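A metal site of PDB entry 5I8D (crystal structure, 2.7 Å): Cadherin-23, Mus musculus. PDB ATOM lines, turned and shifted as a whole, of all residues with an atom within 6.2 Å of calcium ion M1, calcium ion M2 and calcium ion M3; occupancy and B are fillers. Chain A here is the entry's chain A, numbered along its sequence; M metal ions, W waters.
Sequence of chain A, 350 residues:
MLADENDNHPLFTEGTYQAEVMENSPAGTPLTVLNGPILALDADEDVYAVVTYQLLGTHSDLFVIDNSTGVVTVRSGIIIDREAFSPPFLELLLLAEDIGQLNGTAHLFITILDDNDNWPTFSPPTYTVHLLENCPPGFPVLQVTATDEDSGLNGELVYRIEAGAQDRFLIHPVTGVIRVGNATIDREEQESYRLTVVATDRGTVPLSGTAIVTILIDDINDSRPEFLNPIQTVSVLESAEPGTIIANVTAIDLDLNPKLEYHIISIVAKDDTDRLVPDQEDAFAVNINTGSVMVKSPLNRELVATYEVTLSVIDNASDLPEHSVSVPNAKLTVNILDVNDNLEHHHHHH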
ATOM      1  N   GLU A  23      21.099 -19.197 -23.779  1.00  0.00           N
ATOM      2  CA  GLU A  23      19.813 -19.743 -23.318  1.00  0.00           C
ATOM      3  C   GLU A  23      19.253 -18.853 -22.176  1.00  0.00           C
ATOM      4  O   GLU A  23      19.980 -18.049 -21.591  1.00  0.00           O
ATOM      5  CB  GLU A  23      19.939 -21.219 -22.875  1.00  0.00           C
ATOM      6  CG  GLU A  23      20.815 -21.490 -21.636  1.00  0.00           C
ATOM      7  CD  GLU A  23      20.729 -22.926 -21.109  1.00  0.00           C
ATOM      8  OE1 GLU A  23      21.675 -23.323 -20.393  1.00  0.00           O
ATOM      9  OE2 GLU A  23      19.733 -23.649 -21.395  1.00  0.00           O
ATOM     10  N   ASN A  24      17.955 -18.996 -21.906  1.00  0.00           N
ATOM     11  CA  ASN A  24      17.263 -18.225 -20.849  1.00  0.00           C
ATOM     12  C   ASN A  24      17.387 -16.703 -21.071  1.00  0.00           C
ATOM     13  O   ASN A  24      17.303 -15.931 -20.116  1.00  0.00           O
ATOM     14  CB  ASN A  24      17.786 -18.568 -19.437  1.00  0.00           C
ATOM     15  CG  ASN A  24      17.887 -20.066 -19.181  1.00  0.00           C
ATOM     16  OD1 ASN A  24      17.005 -20.848 -19.553  1.00  0.00           O
ATOM     17  ND2 ASN A  24      18.981 -20.476 -18.516  1.00  0.00           N
ATOM     18  N   ILE A  80      13.962 -20.156 -24.191  1.00  0.00           N
ATOM     19  CA  ILE A  80      15.007 -20.858 -24.963  1.00  0.00           C
ATOM     20  C   ILE A  80      15.884 -21.668 -24.001  1.00  0.00           C
ATOM     21  O   ILE A  80      16.691 -21.093 -23.270  1.00  0.00           O
ATOM     22  CB  ILE A  80      15.891 -19.878 -25.791  1.00  0.00           C
ATOM     23  CG1 ILE A  80      15.021 -19.070 -26.766  1.00  0.00           C
ATOM     24  CG2 ILE A  80      16.977 -20.655 -26.547  1.00  0.00           C
ATOM     25  CD1 ILE A  80      15.763 -17.966 -27.492  1.00  0.00           C
ATOM     26  N   ASP A  81      15.724 -23.001 -24.032  1.00  0.00           N
ATOM     27  CA  ASP A  81      16.417 -23.940 -23.107  1.00  0.00           C
ATOM     28  C   ASP A  81      17.345 -24.916 -23.860  1.00  0.00           C
ATOM     29  O   ASP A  81      16.876 -25.919 -24.460  1.00  0.00           O
ATOM     30  CB  ASP A  81      15.377 -24.716 -22.284  1.00  0.00           C
ATOM     31  CG  ASP A  81      15.935 -25.996 -21.654  1.00  0.00           C
ATOM     32  OD1 ASP A  81      17.065 -25.965 -21.112  1.00  0.00           O
ATOM     33  OD2 ASP A  81      15.242 -27.031 -21.698  1.00  0.00           O
ATOM     34  N   ARG A  82      18.645 -24.660 -23.776  1.00  0.00           N
ATOM     35  CA  ARG A  82      19.653 -25.500 -24.451  1.00  0.00           C
ATOM     36  C   ARG A  82      19.405 -27.017 -24.277  1.00  0.00           C
ATOM     37  O   ARG A  82      19.375 -27.775 -25.262  1.00  0.00           O
ATOM     38  CB  ARG A  82      21.063 -25.139 -23.979  1.00  0.00           C
ATOM     39  CG  ARG A  82      22.160 -25.631 -24.906  1.00  0.00           C
ATOM     40  CD  ARG A  82      23.518 -25.580 -24.225  1.00  0.00           C
ATOM     41  NE  ARG A  82      23.662 -26.630 -23.215  1.00  0.00           N
ATOM     42  CZ  ARG A  82      24.022 -27.895 -23.436  1.00  0.00           C
ATOM     43  NH1 ARG A  82      24.113 -28.747 -22.410  1.00  0.00           N
ATOM     44  NH2 ARG A  82      24.298 -28.344 -24.683  1.00  0.00           N
ATOM     45  N   GLU A  83      19.126 -27.404 -23.035  1.00  0.00           N
ATOM     46  CA  GLU A  83      18.864 -28.795 -22.670  1.00  0.00           C
ATOM     47  C   GLU A  83      17.657 -29.458 -23.378  1.00  0.00           C
ATOM     48  O   GLU A  83      17.483 -30.666 -23.218  1.00  0.00           O
ATOM     49  CB  GLU A  83      18.656 -28.921 -21.146  1.00  0.00           C
ATOM     50  CG  GLU A  83      19.940 -28.857 -20.344  1.00  0.00           C
ATOM     51  CD  GLU A  83      20.599 -27.495 -20.387  1.00  0.00           C
ATOM     52  OE1 GLU A  83      19.972 -26.489 -19.963  1.00  0.00           O
ATOM     53  OE2 GLU A  83      21.760 -27.417 -20.840  1.00  0.00           O
ATOM     54  N   ASP A 114      25.514 -22.173 -23.838  1.00  0.00           N
ATOM     55  CA  ASP A 114      25.194 -22.804 -22.535  1.00  0.00           C
ATOM     56  C   ASP A 114      25.283 -21.855 -21.354  1.00  0.00           C
ATOM     57  O   ASP A 114      26.224 -21.068 -21.226  1.00  0.00           O
ATOM     58  CB  ASP A 114      26.097 -24.023 -22.255  1.00  0.00           C
ATOM     59  CG  ASP A 114      25.646 -24.826 -21.011  1.00  0.00           C
ATOM     60  OD1 ASP A 114      24.433 -25.140 -20.882  1.00  0.00           O
ATOM     61  OD2 ASP A 114      26.496 -25.156 -20.154  1.00  0.00           O
ATOM     62  N   ASP A 115      24.281 -21.992 -20.473  1.00  0.00           N
ATOM     63  CA  ASP A 115      24.219 -21.296 -19.191  1.00  0.00           C
ATOM     64  C   ASP A 115      24.208 -22.367 -18.106  1.00  0.00           C
ATOM     65  O   ASP A 115      23.552 -23.388 -18.246  1.00  0.00           O
ATOM     66  CB  ASP A 115      22.943 -20.463 -19.136  1.00  0.00           C
ATOM     67  CG  ASP A 115      22.808 -19.643 -17.876  1.00  0.00           C
ATOM     68  OD1 ASP A 115      23.850 -19.252 -17.286  1.00  0.00           O
ATOM     69  OD2 ASP A 115      21.633 -19.374 -17.496  1.00  0.00           O
ATOM     70  N   ASN A 116      24.932 -22.129 -17.018  1.00  0.00           N
ATOM     71  CA  ASN A 116      25.026 -23.094 -15.933  1.00  0.00           C
ATOM     72  C   ASN A 116      23.753 -23.055 -15.090  1.00  0.00           C
ATOM     73  O   ASN A 116      23.737 -22.474 -14.000  1.00  0.00           O
ATOM     74  CB  ASN A 116      26.270 -22.811 -15.087  1.00  0.00           C
ATOM     75  CG  ASN A 116      26.580 -23.925 -14.111  1.00  0.00           C
ATOM     76  OD1 ASN A 116      26.334 -25.100 -14.386  1.00  0.00           O
ATOM     77  ND2 ASN A 116      27.123 -23.571 -12.956  1.00  0.00           N
ATOM     78  N   ASP A 117      22.686 -23.676 -15.620  1.00  0.00           N
ATOM     79  CA  ASP A 117      21.347 -23.608 -15.008  1.00  0.00           C
ATOM     80  C   ASP A 117      20.791 -24.938 -14.482  1.00  0.00           C
ATOM     81  O   ASP A 117      19.607 -25.036 -14.143  1.00  0.00           O
ATOM     82  CB  ASP A 117      20.343 -22.934 -15.969  1.00  0.00           C
ATOM     83  CG  ASP A 117      20.050 -23.753 -17.210  1.00  0.00           C
ATOM     84  OD1 ASP A 117      20.929 -24.447 -17.756  1.00  0.00           O
ATOM     85  OD2 ASP A 117      18.896 -23.682 -17.674  1.00  0.00           O
ATOM     86  N   ASN A 118      21.672 -25.948 -14.405  1.00  0.00           N
ATOM     87  CA  ASN A 118      21.341 -27.285 -13.866  1.00  0.00           C
ATOM     88  C   ASN A 118      22.318 -27.635 -12.764  1.00  0.00           C
ATOM     89  O   ASN A 118      23.527 -27.510 -12.949  1.00  0.00           O
ATOM     90  CB  ASN A 118      21.413 -28.365 -14.945  1.00  0.00           C
ATOM     91  CG  ASN A 118      20.229 -28.325 -15.894  1.00  0.00           C
ATOM     92  OD1 ASN A 118      19.258 -29.034 -15.695  1.00  0.00           O
ATOM     93  ND2 ASN A 118      20.313 -27.503 -16.930  1.00  0.00           N
ATOM     94  N   TRP A 119      21.788 -28.112 -11.639  1.00  0.00           N
ATOM     95  CA  TRP A 119      22.588 -28.478 -10.474  1.00  0.00           C
ATOM     96  C   TRP A 119      23.168 -29.896 -10.647  1.00  0.00           C
ATOM     97  O   TRP A 119      22.484 -30.774 -11.143  1.00  0.00           O
ATOM     98  CB  TRP A 119      21.739 -28.455  -9.199  1.00  0.00           C
ATOM     99  CG  TRP A 119      21.465 -27.092  -8.611  1.00  0.00           C
ATOM    100  CD1 TRP A 119      22.090 -26.533  -7.538  1.00  0.00           C
ATOM    101  CD2 TRP A 119      20.460 -26.159  -9.023  1.00  0.00           C
ATOM    102  NE1 TRP A 119      21.557 -25.298  -7.274  1.00  0.00           N
ATOM    103  CE2 TRP A 119      20.557 -25.045  -8.166  1.00  0.00           C
ATOM    104  CE3 TRP A 119      19.492 -26.148 -10.048  1.00  0.00           C
ATOM    105  CZ2 TRP A 119      19.716 -23.921  -8.296  1.00  0.00           C
ATOM    106  CZ3 TRP A 119      18.664 -25.033 -10.170  1.00  0.00           C
ATOM    107  CH2 TRP A 119      18.779 -23.935  -9.310  1.00  0.00           C
ATOM    108  N   PRO A 120      24.438 -30.114 -10.230  1.00  0.00           N
ATOM    109  CA  PRO A 120      24.848 -31.502 -10.006  1.00  0.00           C
ATOM    110  C   PRO A 120      23.849 -32.185  -9.055  1.00  0.00           C
ATOM    111  O   PRO A 120      23.682 -31.727  -7.922  1.00  0.00           O
ATOM    112  CB  PRO A 120      26.221 -31.354  -9.331  1.00  0.00           C
ATOM    113  CG  PRO A 120      26.744 -30.045  -9.814  1.00  0.00           C
ATOM    114  CD  PRO A 120      25.558 -29.161 -10.065  1.00  0.00           C
ATOM    115  N   ASP A 148      24.800 -34.080 -14.163  1.00  0.00           N
ATOM    116  CA  ASP A 148      24.589 -32.645 -14.427  1.00  0.00           C
ATOM    117  C   ASP A 148      24.241 -32.475 -15.908  1.00  0.00           C
ATOM    118  O   ASP A 148      25.074 -32.772 -16.775  1.00  0.00           O
ATOM    119  CB  ASP A 148      25.871 -31.864 -14.065  1.00  0.00           C
ATOM    120  CG  ASP A 148      25.702 -30.335 -14.152  1.00  0.00           C
ATOM    121  OD1 ASP A 148      25.053 -29.823 -15.090  1.00  0.00           O
ATOM    122  OD2 ASP A 148      26.251 -29.614 -13.270  1.00  0.00           O
ATOM    123  N   GLU A 149      23.043 -31.969 -16.208  1.00  0.00           N
ATOM    124  CA  GLU A 149      22.575 -31.858 -17.598  1.00  0.00           C
ATOM    125  C   GLU A 149      23.242 -30.726 -18.424  1.00  0.00           C
ATOM    126  O   GLU A 149      22.978 -30.607 -19.613  1.00  0.00           O
ATOM    127  CB  GLU A 149      21.049 -31.692 -17.659  1.00  0.00           C
ATOM    128  CG  GLU A 149      20.227 -32.711 -16.874  1.00  0.00           C
ATOM    129  CD  GLU A 149      20.677 -34.151 -17.055  1.00  0.00           C
ATOM    130  OE1 GLU A 149      21.277 -34.717 -16.110  1.00  0.00           O
ATOM    131  OE2 GLU A 149      20.426 -34.727 -18.140  1.00  0.00           O
ATOM    132  N   ASP A 150      24.077 -29.899 -17.810  1.00  0.00           N
ATOM    133  CA  ASP A 150      24.834 -28.882 -18.556  1.00  0.00           C
ATOM    134  C   ASP A 150      26.052 -29.510 -19.257  1.00  0.00           C
ATOM    135  O   ASP A 150      26.379 -30.695 -19.040  1.00  0.00           O
ATOM    136  CB  ASP A 150      25.282 -27.737 -17.634  1.00  0.00           C
ATOM    137  CG  ASP A 150      24.111 -27.037 -16.952  1.00  0.00           C
ATOM    138  OD1 ASP A 150      23.033 -26.868 -17.583  1.00  0.00           O
ATOM    139  OD2 ASP A 150      24.282 -26.659 -15.768  1.00  0.00           O
ATOM    140  N   SER A 151      26.702 -28.688 -20.087  1.00  0.00           N
ATOM    141  CA  SER A 151      27.849 -29.107 -20.910  1.00  0.00           C
ATOM    142  C   SER A 151      29.139 -28.426 -20.433  1.00  0.00           C
ATOM    143  O   SER A 151      29.149 -27.693 -19.431  1.00  0.00           O
ATOM    144  CB  SER A 151      27.576 -28.777 -22.383  1.00  0.00           C
ATOM    145  OG  SER A 151      27.534 -27.369 -22.595  1.00  0.00           O
ATOM    146  N   LEU A 153      32.424 -27.022 -18.935  1.00  0.00           N
ATOM    147  CA  LEU A 153      32.762 -26.823 -17.535  1.00  0.00           C
ATOM    148  C   LEU A 153      31.504 -26.728 -16.652  1.00  0.00           C
ATOM    149  O   LEU A 153      31.556 -27.004 -15.438  1.00  0.00           O
ATOM    150  CB  LEU A 153      33.643 -25.564 -17.377  1.00  0.00           C
ATOM    151  CG  LEU A 153      35.024 -25.597 -18.068  1.00  0.00           C
ATOM    152  CD1 LEU A 153      35.687 -24.223 -18.054  1.00  0.00           C
ATOM    153  CD2 LEU A 153      35.959 -26.634 -17.469  1.00  0.00           C
ATOM    154  N   ASN A 154      30.373 -26.386 -17.271  1.00  0.00           N
ATOM    155  CA  ASN A 154      29.098 -26.307 -16.547  1.00  0.00           C
ATOM    156  C   ASN A 154      28.566 -27.675 -16.140  1.00  0.00           C
ATOM    157  O   ASN A 154      27.751 -27.767 -15.217  1.00  0.00           O
ATOM    158  CB  ASN A 154      28.047 -25.548 -17.360  1.00  0.00           C
ATOM    159  CG  ASN A 154      28.484 -24.132 -17.686  1.00  0.00           C
ATOM    160  OD1 ASN A 154      29.463 -23.603 -17.156  1.00  0.00           O
ATOM    161  ND2 ASN A 154      27.731 -23.482 -18.570  1.00  0.00           N
ATOM    162  N   GLY A 155      29.018 -28.738 -16.831  1.00  0.00           N
ATOM    163  CA  GLY A 155      28.682 -30.130 -16.488  1.00  0.00           C
ATOM    164  C   GLY A 155      29.785 -31.006 -15.904  1.00  0.00           C
ATOM    165  O   GLY A 155      29.540 -32.165 -15.587  1.00  0.00           O
ATOM    166  N   LEU A 157      32.343 -32.267 -13.115  1.00  0.00           N
ATOM    167  CA  LEU A 157      32.164 -32.294 -11.655  1.00  0.00           C
ATOM    168  C   LEU A 157      33.443 -32.645 -10.877  1.00  0.00           C
ATOM    169  O   LEU A 157      34.141 -33.607 -11.214  1.00  0.00           O
ATOM    170  CB  LEU A 157      31.051 -33.287 -11.289  1.00  0.00           C
ATOM    171  CG  LEU A 157      29.773 -33.169 -12.138  1.00  0.00           C
ATOM    172  CD1 LEU A 157      28.717 -34.224 -11.782  1.00  0.00           C
ATOM    173  CD2 LEU A 157      29.204 -31.756 -12.038  1.00  0.00           C
ATOM    174  N   ASP A 201      30.135 -28.390  -9.854  1.00  0.00           N
ATOM    175  CA  ASP A 201      30.494 -28.132 -11.270  1.00  0.00           C
ATOM    176  C   ASP A 201      31.480 -26.963 -11.437  1.00  0.00           C
ATOM    177  O   ASP A 201      31.835 -26.307 -10.454  1.00  0.00           O
ATOM    178  CB  ASP A 201      29.241 -27.992 -12.173  1.00  0.00           C
ATOM    179  CG  ASP A 201      28.485 -26.674 -11.980  1.00  0.00           C
ATOM    180  OD1 ASP A 201      29.090 -25.654 -11.593  1.00  0.00           O
ATOM    181  OD2 ASP A 201      27.263 -26.667 -12.253  1.00  0.00           O
ATOM    182  N   LEU A 207      27.822 -24.440  -9.307  1.00  0.00           N
ATOM    183  CA  LEU A 207      26.691 -25.066  -8.601  1.00  0.00           C
ATOM    184  C   LEU A 207      27.121 -26.417  -8.035  1.00  0.00           C
ATOM    185  O   LEU A 207      27.931 -27.149  -8.652  1.00  0.00           O
ATOM    186  CB  LEU A 207      25.459 -25.263  -9.510  1.00  0.00           C
ATOM    187  CG  LEU A 207      24.712 -24.026 -10.048  1.00  0.00           C
ATOM    188  CD1 LEU A 207      23.541 -24.427 -10.928  1.00  0.00           C
ATOM    189  CD2 LEU A 207      24.226 -23.137  -8.908  1.00  0.00           C
HETATM  190 CA    CA M   1      22.380 -25.314 -19.410  1.00  0.00          CA
HETATM  191 CA    CA M   2      18.276 -24.619 -19.654  1.00  0.00          CA
HETATM  192 CA    CA M   3      25.661 -27.287 -13.856  1.00  0.00          CA
HETATM  193  O   HOH W   1      17.771 -26.308 -18.248  1.00  0.00           O
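The backbone carbonyl oxygen (O) of Asn 118 binds calcium ion M3 (2.3 Å).
Calcium ion M3 is bound by OD1 of Asn 116, at 2.3 Å.
Calcium ion M3 is bound by OD2 of Asp 201 (2.3 Å).
The side-chain carboxylate (OD2) of Asp 150 binds calcium ion M3.
The side-chain carboxylate (OD2) of Asp 148 binds calcium ion M3, at 2.5 Å.
O of Asn 154 binds calcium ion M3 (2.5 Å).
OD1 of Asp 148 binds calcium ion M3, 2.9 Å away.
Calcium ion M3 has seven donor atoms within binding distance.
Within 4 Å of calcium ion M3: Asn 116, Asn 118, Asp 148, Asp 150, Asn 154 and Asp 201.
Along chain A the residues within 4 Å of calcium ion M3 span positions 116 to 201.
Calcium ion M1 is bound by OE1 of Glu 23, OD1 of Asp 117, OD1 of Asp 150, OD1 of Asp 114, O of Asp 115, OE2 of Glu 83 and OE1 of Glu 83.
The side-chain carboxylate of Asp 117 sits close to the side-chain amide nitrogen of Asn 118, 3.2 Å away.
OE1 of Glu 83 lies close to ND2 of Asn 118 (3.2 Å).
O of Leu 207 sits at hydrogen-bond distance from N of Asp 201 (2.8 Å).
The side-chain carboxylate (OD2) of Asp 114 sits at hydrogen-bond distance from the side-chain amide nitrogen (ND2) of Asn 154, at 2.6 Å.
The side-chain carboxylate of Asp 114 sits close to the guanidinium group of Arg 82 (2.9 Å).
The side-chain hydroxyl (OG) of Ser 151 sits at hydrogen-bond distance from the side-chain carboxylate (OD2) of Asp 114 (3.5 Å).
The guanidinium group (NH1) of Arg 82 lies close to the side-chain carboxylate (OE2) of Glu 83, 3.1 Å away.
O of Ile 80 sits at hydrogen-bond distance from N of Asn 24 (2.8 Å).
Residues that only touch calcium ion M2: Asn 24 (3.98 Å).
Of the 23 residues printed, 5 come within 4 Å of calcium ion M2.
Water W1 binds calcium ion M2, 2.3 Å away.
Calcium ion M2 is bound by the side-chain carboxylate (OD2) of Asp 117 (2.3 Å).
The side-chain carboxylate (OD1) of Asp 81 binds calcium ion M2, at 2.3 Å.
OE2 of Glu 23 is bound to calcium ion M2.
The side-chain carboxylate (OE1) of Glu 83 binds calcium ion M2 (2.5 Å).
Calcium ion M2 has five donor atoms within binding distance.
Seven residues have an atom within 4 Å of calcium ion M1: Glu 23, Glu 83, Asp 114, Asp 115, Asp 117, Asn 118 and Asp 150.
The nearest printed residue that does not touch calcium ion M1 is Arg 82 (4.2 Å).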
